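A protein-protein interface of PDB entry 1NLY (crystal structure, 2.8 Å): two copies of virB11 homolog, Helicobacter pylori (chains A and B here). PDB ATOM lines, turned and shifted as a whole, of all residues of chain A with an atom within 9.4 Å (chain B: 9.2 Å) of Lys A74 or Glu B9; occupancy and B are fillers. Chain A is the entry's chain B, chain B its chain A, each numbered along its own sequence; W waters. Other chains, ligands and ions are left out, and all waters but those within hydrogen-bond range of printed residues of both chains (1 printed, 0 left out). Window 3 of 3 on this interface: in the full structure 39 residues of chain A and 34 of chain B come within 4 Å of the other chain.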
ATOM      1  N   ALA A  31      -7.418  18.699  20.036  1.00  0.00           N
ATOM      2  CA  ALA A  31      -6.037  18.537  20.478  1.00  0.00           C
ATOM      3  C   ALA A  31      -5.289  19.811  20.135  1.00  0.00           C
ATOM      4  O   ALA A  31      -4.627  20.409  20.982  1.00  0.00           O
ATOM      5  CB  ALA A  31      -5.391  17.357  19.787  1.00  0.00           C
ATOM      6  N   GLU A  34      -6.500  22.508  22.229  1.00  0.00           N
ATOM      7  CA  GLU A  34      -6.008  22.219  23.564  1.00  0.00           C
ATOM      8  C   GLU A  34      -4.566  22.605  23.808  1.00  0.00           C
ATOM      9  O   GLU A  34      -4.258  23.193  24.838  1.00  0.00           O
ATOM     10  CB  GLU A  34      -6.204  20.732  23.867  1.00  0.00           C
ATOM     11  CG  GLU A  34      -5.219  20.137  24.859  1.00  0.00           C
ATOM     12  CD  GLU A  34      -5.274  18.599  24.907  1.00  0.00           C
ATOM     13  OE1 GLU A  34      -5.199  17.968  23.827  1.00  0.00           O
ATOM     14  OE2 GLU A  34      -5.385  18.023  26.019  1.00  0.00           O
ATOM     15  N   LEU A  35      -3.685  22.287  22.865  1.00  0.00           N
ATOM     16  CA  LEU A  35      -2.262  22.590  23.021  1.00  0.00           C
ATOM     17  C   LEU A  35      -1.849  23.958  22.505  1.00  0.00           C
ATOM     18  O   LEU A  35      -1.621  24.889  23.277  1.00  0.00           O
ATOM     19  CB  LEU A  35      -1.406  21.546  22.308  1.00  0.00           C
ATOM     20  CG  LEU A  35      -1.174  20.219  23.007  1.00  0.00           C
ATOM     21  CD1 LEU A  35      -2.472  19.529  23.258  1.00  0.00           C
ATOM     22  CD2 LEU A  35      -0.306  19.365  22.135  1.00  0.00           C
ATOM     23  N   TYR A  50       8.147  23.478  19.600  1.00  0.00           N
ATOM     24  CA  TYR A  50       8.129  22.872  20.925  1.00  0.00           C
ATOM     25  C   TYR A  50       9.290  21.901  20.963  1.00  0.00           C
ATOM     26  O   TYR A  50       9.393  21.001  20.121  1.00  0.00           O
ATOM     27  CB  TYR A  50       6.831  22.149  21.210  1.00  0.00           C
ATOM     28  CG  TYR A  50       6.779  21.656  22.644  1.00  0.00           C
ATOM     29  CD1 TYR A  50       6.850  22.549  23.720  1.00  0.00           C
ATOM     30  CD2 TYR A  50       6.714  20.287  22.930  1.00  0.00           C
ATOM     31  CE1 TYR A  50       6.862  22.078  25.068  1.00  0.00           C
ATOM     32  CE2 TYR A  50       6.730  19.800  24.260  1.00  0.00           C
ATOM     33  CZ  TYR A  50       6.805  20.694  25.323  1.00  0.00           C
ATOM     34  OH  TYR A  50       6.854  20.197  26.608  1.00  0.00           O
ATOM     35  N   LYS A  54       9.091  21.571  27.986  1.00  0.00           N
ATOM     36  CA  LYS A  54       8.094  22.392  28.675  1.00  0.00           C
ATOM     37  C   LYS A  54       8.043  23.888  28.305  1.00  0.00           C
ATOM     38  O   LYS A  54       7.419  24.694  28.998  1.00  0.00           O
ATOM     39  CB  LYS A  54       8.280  22.241  30.188  1.00  0.00           C
ATOM     40  CG  LYS A  54       8.183  20.810  30.677  1.00  0.00           C
ATOM     41  CD  LYS A  54       6.825  20.244  30.328  1.00  0.00           C
ATOM     42  CE  LYS A  54       6.653  18.839  30.893  1.00  0.00           C
ATOM     43  NZ  LYS A  54       5.221  18.373  30.880  1.00  0.00           N
ATOM     44  N   VAL A  70       5.115  26.480  29.905  1.00  0.00           N
ATOM     45  CA  VAL A  70       3.914  25.623  29.970  1.00  0.00           C
ATOM     46  C   VAL A  70       4.125  24.461  30.933  1.00  0.00           C
ATOM     47  O   VAL A  70       3.471  23.417  30.850  1.00  0.00           O
ATOM     48  CB  VAL A  70       3.527  25.029  28.590  1.00  0.00           C
ATOM     49  CG1 VAL A  70       2.980  26.108  27.696  1.00  0.00           C
ATOM     50  CG2 VAL A  70       4.724  24.345  27.949  1.00  0.00           C
ATOM     51  N   ARG A  71       5.058  24.666  31.846  1.00  0.00           N
ATOM     52  CA  ARG A  71       5.400  23.683  32.858  1.00  0.00           C
ATOM     53  C   ARG A  71       4.143  23.158  33.550  1.00  0.00           C
ATOM     54  O   ARG A  71       4.030  21.964  33.854  1.00  0.00           O
ATOM     55  CB  ARG A  71       6.298  24.337  33.903  1.00  0.00           C
ATOM     56  CG  ARG A  71       7.517  23.544  34.283  1.00  0.00           C
ATOM     57  CD  ARG A  71       8.276  24.284  35.386  1.00  0.00           C
ATOM     58  NE  ARG A  71       8.413  25.715  35.093  1.00  0.00           N
ATOM     59  CZ  ARG A  71       9.284  26.530  35.691  1.00  0.00           C
ATOM     60  NH1 ARG A  71      10.097  26.047  36.621  1.00  0.00           N
ATOM     61  NH2 ARG A  71       9.361  27.818  35.346  1.00  0.00           N
ATOM     62  N   ASP A  72       3.202  24.063  33.796  1.00  0.00           N
ATOM     63  CA  ASP A  72       1.972  23.727  34.498  1.00  0.00           C
ATOM     64  C   ASP A  72       0.770  23.746  33.570  1.00  0.00           C
ATOM     65  O   ASP A  72      -0.108  24.595  33.706  1.00  0.00           O
ATOM     66  CB  ASP A  72       1.745  24.724  35.648  1.00  0.00           C
ATOM     67  CG  ASP A  72       2.996  24.918  36.516  1.00  0.00           C
ATOM     68  OD1 ASP A  72       3.459  23.918  37.111  1.00  0.00           O
ATOM     69  OD2 ASP A  72       3.519  26.062  36.596  1.00  0.00           O
ATOM     70  N   ARG A  73       0.741  22.814  32.626  1.00  0.00           N
ATOM     71  CA  ARG A  73      -0.365  22.704  31.684  1.00  0.00           C
ATOM     72  C   ARG A  73      -0.501  21.233  31.390  1.00  0.00           C
ATOM     73  O   ARG A  73       0.507  20.557  31.181  1.00  0.00           O
ATOM     74  CB  ARG A  73      -0.062  23.422  30.372  1.00  0.00           C
ATOM     75  CG  ARG A  73      -0.154  24.933  30.408  1.00  0.00           C
ATOM     76  CD  ARG A  73      -0.838  25.437  29.135  1.00  0.00           C
ATOM     77  NE  ARG A  73      -0.714  26.881  28.939  1.00  0.00           N
ATOM     78  CZ  ARG A  73      -1.175  27.525  27.872  1.00  0.00           C
ATOM     79  NH1 ARG A  73      -1.799  26.845  26.918  1.00  0.00           N
ATOM     80  NH2 ARG A  73      -0.978  28.831  27.737  1.00  0.00           N
ATOM     81  N   LYS A  74      -1.739  20.749  31.364  1.00  0.00           N
ATOM     82  CA  LYS A  74      -2.027  19.342  31.098  1.00  0.00           C
ATOM     83  C   LYS A  74      -1.777  19.018  29.625  1.00  0.00           C
ATOM     84  O   LYS A  74      -1.278  17.938  29.287  1.00  0.00           O
ATOM     85  CB  LYS A  74      -3.487  19.039  31.482  1.00  0.00           C
ATOM     86  CG  LYS A  74      -4.021  17.654  31.096  1.00  0.00           C
ATOM     87  CD  LYS A  74      -3.595  16.533  32.059  1.00  0.00           C
ATOM     88  CE  LYS A  74      -4.397  15.224  31.794  1.00  0.00           C
ATOM     89  NZ  LYS A  74      -4.207  14.120  32.809  1.00  0.00           N
ATOM     90  N   ALA A  75      -2.111  19.976  28.760  1.00  0.00           N
ATOM     91  CA  ALA A  75      -1.955  19.816  27.313  1.00  0.00           C
ATOM     92  C   ALA A  75      -0.533  19.475  26.914  1.00  0.00           C
ATOM     93  O   ALA A  75      -0.271  19.127  25.766  1.00  0.00           O
ATOM     94  CB  ALA A  75      -2.414  21.086  26.571  1.00  0.00           C
ATOM     95  N   PHE A  76       0.387  19.576  27.860  1.00  0.00           N
ATOM     96  CA  PHE A  76       1.765  19.246  27.564  1.00  0.00           C
ATOM     97  C   PHE A  76       2.288  18.079  28.396  1.00  0.00           C
ATOM     98  O   PHE A  76       3.347  18.151  29.020  1.00  0.00           O
ATOM     99  CB  PHE A  76       2.635  20.490  27.707  1.00  0.00           C
ATOM    100  CG  PHE A  76       2.444  21.466  26.579  1.00  0.00           C
ATOM    101  CD1 PHE A  76       1.329  22.295  26.530  1.00  0.00           C
ATOM    102  CD2 PHE A  76       3.351  21.514  25.525  1.00  0.00           C
ATOM    103  CE1 PHE A  76       1.118  23.144  25.440  1.00  0.00           C
ATOM    104  CE2 PHE A  76       3.146  22.360  24.431  1.00  0.00           C
ATOM    105  CZ  PHE A  76       2.029  23.179  24.392  1.00  0.00           C
ATOM    106  N   SER A  77       1.512  16.999  28.385  1.00  0.00           N
ATOM    107  CA  SER A  77       1.852  15.772  29.087  1.00  0.00           C
ATOM    108  C   SER A  77       2.313  14.796  28.003  1.00  0.00           C
ATOM    109  O   SER A  77       1.737  14.774  26.911  1.00  0.00           O
ATOM    110  CB  SER A  77       0.609  15.227  29.790  1.00  0.00           C
ATOM    111  OG  SER A  77      -0.037  16.270  30.496  1.00  0.00           O
ATOM    112  N   LEU A  78       3.350  14.008  28.256  1.00  0.00           N
ATOM    113  CA  LEU A  78       3.774  13.074  27.224  1.00  0.00           C
ATOM    114  C   LEU A  78       2.563  12.422  26.522  1.00  0.00           C
ATOM    115  O   LEU A  78       2.536  12.299  25.299  1.00  0.00           O
ATOM    116  CB  LEU A  78       4.693  12.007  27.824  1.00  0.00           C
ATOM    117  CG  LEU A  78       6.059  12.500  28.309  1.00  0.00           C
ATOM    118  CD1 LEU A  78       6.877  11.350  28.880  1.00  0.00           C
ATOM    119  CD2 LEU A  78       6.786  13.119  27.154  1.00  0.00           C
ATOM    120  N   SER A  79       1.546  12.039  27.289  1.00  0.00           N
ATOM    121  CA  SER A  79       0.357  11.407  26.702  1.00  0.00           C
ATOM    122  C   SER A  79      -0.460  12.393  25.877  1.00  0.00           C
ATOM    123  O   SER A  79      -0.737  12.143  24.708  1.00  0.00           O
ATOM    124  CB  SER A  79      -0.539  10.802  27.785  1.00  0.00           C
ATOM    125  OG  SER A  79      -1.104  11.819  28.583  1.00  0.00           O
ATOM    126  N   ARG A  80      -0.849  13.507  26.497  1.00  0.00           N
ATOM    127  CA  ARG A  80      -1.610  14.574  25.837  1.00  0.00           C
ATOM    128  C   ARG A  80      -0.930  15.022  24.533  1.00  0.00           C
ATOM    129  O   ARG A  80      -1.596  15.387  23.557  1.00  0.00           O
ATOM    130  CB  ARG A  80      -1.730  15.782  26.780  1.00  0.00           C
ATOM    131  CG  ARG A  80      -2.741  15.650  27.925  1.00  0.00           C
ATOM    132  CD  ARG A  80      -4.173  15.640  27.380  1.00  0.00           C
ATOM    133  NE  ARG A  80      -4.534  14.340  26.798  1.00  0.00           N
ATOM    134  CZ  ARG A  80      -5.402  14.161  25.797  1.00  0.00           C
ATOM    135  NH1 ARG A  80      -6.003  15.206  25.240  1.00  0.00           N
ATOM    136  NH2 ARG A  80      -5.697  12.930  25.371  1.00  0.00           N
ATOM    137  N   LEU A  81       0.401  15.012  24.531  1.00  0.00           N
ATOM    138  CA  LEU A  81       1.167  15.399  23.356  1.00  0.00           C
ATOM    139  C   LEU A  81       1.072  14.310  22.288  1.00  0.00           C
ATOM    140  O   LEU A  81       0.823  14.586  21.112  1.00  0.00           O
ATOM    141  CB  LEU A  81       2.632  15.621  23.735  1.00  0.00           C
ATOM    142  CG  LEU A  81       3.064  16.976  24.323  1.00  0.00           C
ATOM    143  CD1 LEU A  81       4.494  16.853  24.836  1.00  0.00           C
ATOM    144  CD2 LEU A  81       2.995  18.080  23.270  1.00  0.00           C
ATOM    145  N   MET A  82       1.268  13.066  22.712  1.00  0.00           N
ATOM    146  CA  MET A  82       1.207  11.933  21.803  1.00  0.00           C
ATOM    147  C   MET A  82      -0.165  11.817  21.123  1.00  0.00           C
ATOM    148  O   MET A  82      -0.261  11.533  19.927  1.00  0.00           O
ATOM    149  CB  MET A  82       1.522  10.654  22.570  1.00  0.00           C
ATOM    150  CG  MET A  82       2.092   9.573  21.685  1.00  0.00           C
ATOM    151  SD  MET A  82       3.544  10.345  20.671  1.00  0.00           S
ATOM    152  CE  MET A  82       4.927  10.322  22.050  1.00  0.00           C
ATOM    153  N   HIS A  83      -1.229  12.030  21.888  1.00  0.00           N
ATOM    154  CA  HIS A  83      -2.569  11.963  21.326  1.00  0.00           C
ATOM    155  C   HIS A  83      -2.694  12.991  20.201  1.00  0.00           C
ATOM    156  O   HIS A  83      -3.306  12.718  19.168  1.00  0.00           O
ATOM    157  CB  HIS A  83      -3.611  12.248  22.414  1.00  0.00           C
ATOM    158  CG  HIS A  83      -5.017  12.315  21.903  1.00  0.00           C
ATOM    159  ND1 HIS A  83      -5.757  11.191  21.598  1.00  0.00           N
ATOM    160  CD2 HIS A  83      -5.806  13.376  21.603  1.00  0.00           C
ATOM    161  CE1 HIS A  83      -6.937  11.558  21.126  1.00  0.00           C
ATOM    162  NE2 HIS A  83      -6.990  12.878  21.118  1.00  0.00           N
ATOM    163  N   GLU A 126      11.442  11.635  26.508  1.00  0.00           N
ATOM    164  CA  GLU A 126      10.516  12.610  27.082  1.00  0.00           C
ATOM    165  C   GLU A 126      10.515  13.855  26.212  1.00  0.00           C
ATOM    166  O   GLU A 126       9.865  14.856  26.527  1.00  0.00           O
ATOM    167  CB  GLU A 126      10.943  13.000  28.495  1.00  0.00           C
ATOM    168  CG  GLU A 126      11.254  11.842  29.412  1.00  0.00           C
ATOM    169  CD  GLU A 126      11.315  12.273  30.864  1.00  0.00           C
ATOM    170  OE1 GLU A 126      10.268  12.718  31.391  1.00  0.00           O
ATOM    171  OE2 GLU A 126      12.401  12.169  31.473  1.00  0.00           O
ATOM    172  N   LEU B   6       1.750  15.852  36.051  1.00  0.00           N
ATOM    173  CA  LEU B   6       2.109  15.319  34.698  1.00  0.00           C
ATOM    174  C   LEU B   6       3.103  14.147  34.781  1.00  0.00           C
ATOM    175  O   LEU B   6       2.930  13.121  34.109  1.00  0.00           O
ATOM    176  CB  LEU B   6       2.700  16.445  33.834  1.00  0.00           C
ATOM    177  CG  LEU B   6       1.913  17.764  33.805  1.00  0.00           C
ATOM    178  CD1 LEU B   6       2.668  18.805  32.936  1.00  0.00           C
ATOM    179  CD2 LEU B   6       0.480  17.497  33.284  1.00  0.00           C
ATOM    180  N   SER B   7       4.142  14.306  35.601  1.00  0.00           N
ATOM    181  CA  SER B   7       5.149  13.265  35.762  1.00  0.00           C
ATOM    182  C   SER B   7       4.506  11.933  36.145  1.00  0.00           C
ATOM    183  O   SER B   7       4.943  10.891  35.680  1.00  0.00           O
ATOM    184  CB  SER B   7       6.189  13.665  36.820  1.00  0.00           C
ATOM    185  OG  SER B   7       7.485  13.235  36.427  1.00  0.00           O
ATOM    186  N   ALA B   8       3.464  11.970  36.976  1.00  0.00           N
ATOM    187  CA  ALA B   8       2.768  10.743  37.410  1.00  0.00           C
ATOM    188  C   ALA B   8       2.176  10.021  36.210  1.00  0.00           C
ATOM    189  O   ALA B   8       2.217   8.784  36.128  1.00  0.00           O
ATOM    190  CB  ALA B   8       1.660  11.070  38.424  1.00  0.00           C
ATOM    191  N   GLU B   9       1.614  10.798  35.286  1.00  0.00           N
ATOM    192  CA  GLU B   9       1.049  10.223  34.073  1.00  0.00           C
ATOM    193  C   GLU B   9       2.158   9.918  33.050  1.00  0.00           C
ATOM    194  O   GLU B   9       2.113   8.884  32.375  1.00  0.00           O
ATOM    195  CB  GLU B   9      -0.005  11.155  33.442  1.00  0.00           C
ATOM    196  CG  GLU B   9      -1.273  11.363  34.272  1.00  0.00           C
ATOM    197  CD  GLU B   9      -1.180  12.581  35.177  1.00  0.00           C
ATOM    198  OE1 GLU B   9      -1.171  13.703  34.624  1.00  0.00           O
ATOM    199  OE2 GLU B   9      -1.110  12.424  36.422  1.00  0.00           O
ATOM    200  N   ASP B  10       3.149  10.807  32.947  1.00  0.00           N
ATOM    201  CA  ASP B  10       4.257  10.617  32.006  1.00  0.00           C
ATOM    202  C   ASP B  10       4.951   9.296  32.313  1.00  0.00           C
ATOM    203  O   ASP B  10       5.344   8.572  31.404  1.00  0.00           O
ATOM    204  CB  ASP B  10       5.257  11.797  32.068  1.00  0.00           C
ATOM    205  CG  ASP B  10       4.634  13.125  31.613  1.00  0.00           C
ATOM    206  OD1 ASP B  10       3.592  13.088  30.917  1.00  0.00           O
ATOM    207  OD2 ASP B  10       5.191  14.201  31.950  1.00  0.00           O
ATOM    208  N   LYS B  11       5.065   8.974  33.597  1.00  0.00           N
ATOM    209  CA  LYS B  11       5.686   7.720  34.021  1.00  0.00           C
ATOM    210  C   LYS B  11       4.838   6.515  33.590  1.00  0.00           C
ATOM    211  O   LYS B  11       5.335   5.552  33.003  1.00  0.00           O
ATOM    212  CB  LYS B  11       5.874   7.719  35.543  1.00  0.00           C
ATOM    213  CG  LYS B  11       6.898   8.752  36.041  1.00  0.00           C
ATOM    214  CD  LYS B  11       6.879   8.886  37.577  1.00  0.00           C
ATOM    215  CE  LYS B  11       7.943   9.874  38.095  1.00  0.00           C
ATOM    216  NZ  LYS B  11       7.945  10.011  39.596  1.00  0.00           N
ATOM    217  N   LYS B  12       3.550   6.562  33.881  1.00  0.00           N
ATOM    218  CA  LYS B  12       2.691   5.475  33.473  1.00  0.00           C
ATOM    219  C   LYS B  12       2.639   5.392  31.945  1.00  0.00           C
ATOM    220  O   LYS B  12       2.388   4.327  31.373  1.00  0.00           O
ATOM    221  CB  LYS B  12       1.308   5.701  34.057  1.00  0.00           C
ATOM    222  CG  LYS B  12       1.280   5.533  35.587  1.00  0.00           C
ATOM    223  CD  LYS B  12      -0.011   6.126  36.230  1.00  0.00           C
ATOM    224  CE  LYS B  12      -0.186   5.841  37.752  1.00  0.00           C
ATOM    225  NZ  LYS B  12      -0.651   4.444  38.057  1.00  0.00           N
ATOM    226  N   PHE B  13       2.884   6.519  31.288  1.00  0.00           N
ATOM    227  CA  PHE B  13       2.865   6.551  29.833  1.00  0.00           C
ATOM    228  C   PHE B  13       4.146   5.979  29.231  1.00  0.00           C
ATOM    229  O   PHE B  13       4.125   5.383  28.154  1.00  0.00           O
ATOM    230  CB  PHE B  13       2.701   7.980  29.341  1.00  0.00           C
ATOM    231  CG  PHE B  13       2.780   8.119  27.838  1.00  0.00           C
ATOM    232  CD1 PHE B  13       1.767   7.618  27.032  1.00  0.00           C
ATOM    233  CD2 PHE B  13       3.864   8.760  27.232  1.00  0.00           C
ATOM    234  CE1 PHE B  13       1.829   7.749  25.640  1.00  0.00           C
ATOM    235  CE2 PHE B  13       3.936   8.896  25.835  1.00  0.00           C
ATOM    236  CZ  PHE B  13       2.914   8.391  25.040  1.00  0.00           C
ATOM    237  N   LEU B  14       5.264   6.188  29.916  1.00  0.00           N
ATOM    238  CA  LEU B  14       6.562   5.695  29.457  1.00  0.00           C
ATOM    239  C   LEU B  14       6.758   4.238  29.891  1.00  0.00           C
ATOM    240  O   LEU B  14       7.479   3.452  29.267  1.00  0.00           O
ATOM    241  CB  LEU B  14       7.676   6.577  30.041  1.00  0.00           C
ATOM    242  CG  LEU B  14       7.762   8.030  29.558  1.00  0.00           C
ATOM    243  CD1 LEU B  14       8.605   8.853  30.521  1.00  0.00           C
ATOM    244  CD2 LEU B  14       8.351   8.061  28.166  1.00  0.00           C
ATOM    245  N   GLU B  15       6.077   3.887  30.967  1.00  0.00           N
ATOM    246  CA  GLU B  15       6.169   2.563  31.531  1.00  0.00           C
ATOM    247  C   GLU B  15       6.440   1.449  30.540  1.00  0.00           C
ATOM    248  O   GLU B  15       7.412   0.720  30.698  1.00  0.00           O
ATOM    249  CB  GLU B  15       4.891   2.256  32.307  1.00  0.00           C
ATOM    250  CG  GLU B  15       4.822   0.831  32.879  1.00  0.00           C
ATOM    251  CD  GLU B  15       3.599   0.568  33.812  1.00  0.00           C
ATOM    252  OE1 GLU B  15       2.444   0.781  33.365  1.00  0.00           O
ATOM    253  OE2 GLU B  15       3.793   0.131  34.981  1.00  0.00           O
ATOM    254  N   VAL B  16       5.593   1.322  29.520  1.00  0.00           N
ATOM    255  CA  VAL B  16       5.735   0.247  28.523  1.00  0.00           C
ATOM    256  C   VAL B  16       7.028   0.245  27.727  1.00  0.00           C
ATOM    257  O   VAL B  16       7.684  -0.794  27.577  1.00  0.00           O
ATOM    258  CB  VAL B  16       4.597   0.254  27.473  1.00  0.00           C
ATOM    259  CG1 VAL B  16       4.901  -0.801  26.376  1.00  0.00           C
ATOM    260  CG2 VAL B  16       3.263  -0.023  28.143  1.00  0.00           C
HETATM  261  O   HOH W   1       8.296  12.213  33.590  1.00  0.00           O
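The backbone NH (N) of Lys A54 sits at hydrogen-bond distance from the side-chain hydroxyl (OH) of Tyr A50 (3.0 Å).
The backbone carbonyl oxygen (O) of Lys A54 lies close to the backbone NH (N) of Val A70, at 3.1 Å.
The side-chain amino group of Lys A54 sits at hydrogen-bond distance from the backbone carbonyl oxygen of Phe A76, at 2.6 Å.
The side-chain hydroxyl (OG) of Ser A77 lies within hydrogen-bond range of the backbone carbonyl oxygen (O) of Lys A74.
Of the 11 printed residues of chain B, 5 touch a printed residue of chain A.
Printed residues of chain B that touch a printed residue of chain A: Leu B6, Glu B9, Asp B10, Phe B13 and Leu B14.
Printed residues of chain A that touch a printed residue of chain B: Lys A54, Arg A71, Arg A73, Lys A74, Ser A77, Leu A78 and Met A82.
Hydrophobic or aromatic side chains of chain A within 4 Å of the printed part of chain B: Leu A78 and Met A82.
Among the printed residues, 11 pairs touch across the chains.
Among the printed residues, Asp or Glu carboxylates within 4 Å of a Lys or Arg side-chain nitrogen of the other chain: Lys A74 with Glu B9 (3.6 Å).
Of chain B, only Leu B6 and Glu B9 come within 4 Å of Lys A74.
Glu B9 touches one residue of chain A.
Printed residues of chain B within 4 Å of Ser A77: Leu B6 and Asp B10.
Leu B6 touches just these residues of chain A: Lys A54, Arg A71, Arg A73, Lys A74 and Ser A77.
No residue of chain A comes within 4 Å of Ala B8.
Printed residues of chain B within 4 Å of Arg A73: Leu B6.
Of the printed residues of chain B, Met A82 touches Phe B13.
Printed residues of chain A within 4 Å of Asp B10: Ser A77 and Leu A78.
Of the printed residues of chain B, Leu A78 touches Asp B10, Phe B13 and Leu B14.
Printed residues of chain B within 4 Å of Lys A54: Leu B6.
The nearest residue of chain B that does not touch Lys A74 is Asp B10 (7.1 Å).
The nearest printed residue of chain B that does not touch Met A82 is Leu B14 (7.4 Å).
No position is printed for both chains.
Of the 11 pairs that touch across the chains among the printed residues, none has its exchanged pair printed and touching as well.
Lys A54 touches Leu B6.
Arg A71 touches Leu B6.
Leu B6 touches Arg A73.
CA of Lys A74 touches CD2 of Leu B6, 3.8 Å away.
Leu B6 touches Ser A77.
C of Ser A77 touches OD1 of Asp B10 (3.6 Å).
CB of Leu A78 touches CD2 of Phe B13, at 3.4 Å.
Leu A78 touches Leu B14 (CD1 to CD1, 3.5 Å).
CZ of Phe B13 touches CB of Met A82, at 3.6 Å.
The side-chain amino group of Lys A74 lies within salt-bridge range of the side-chain carboxylate of Glu B9, at 3.6 Å.
The side-chain carboxylate of Asp B10 lies within hydrogen-bond range of the backbone NH of Leu A78, 2.8 Å away.
Water W1 lies within hydrogen-bond range of OE1 of Glu A126 and OG of Ser B7.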
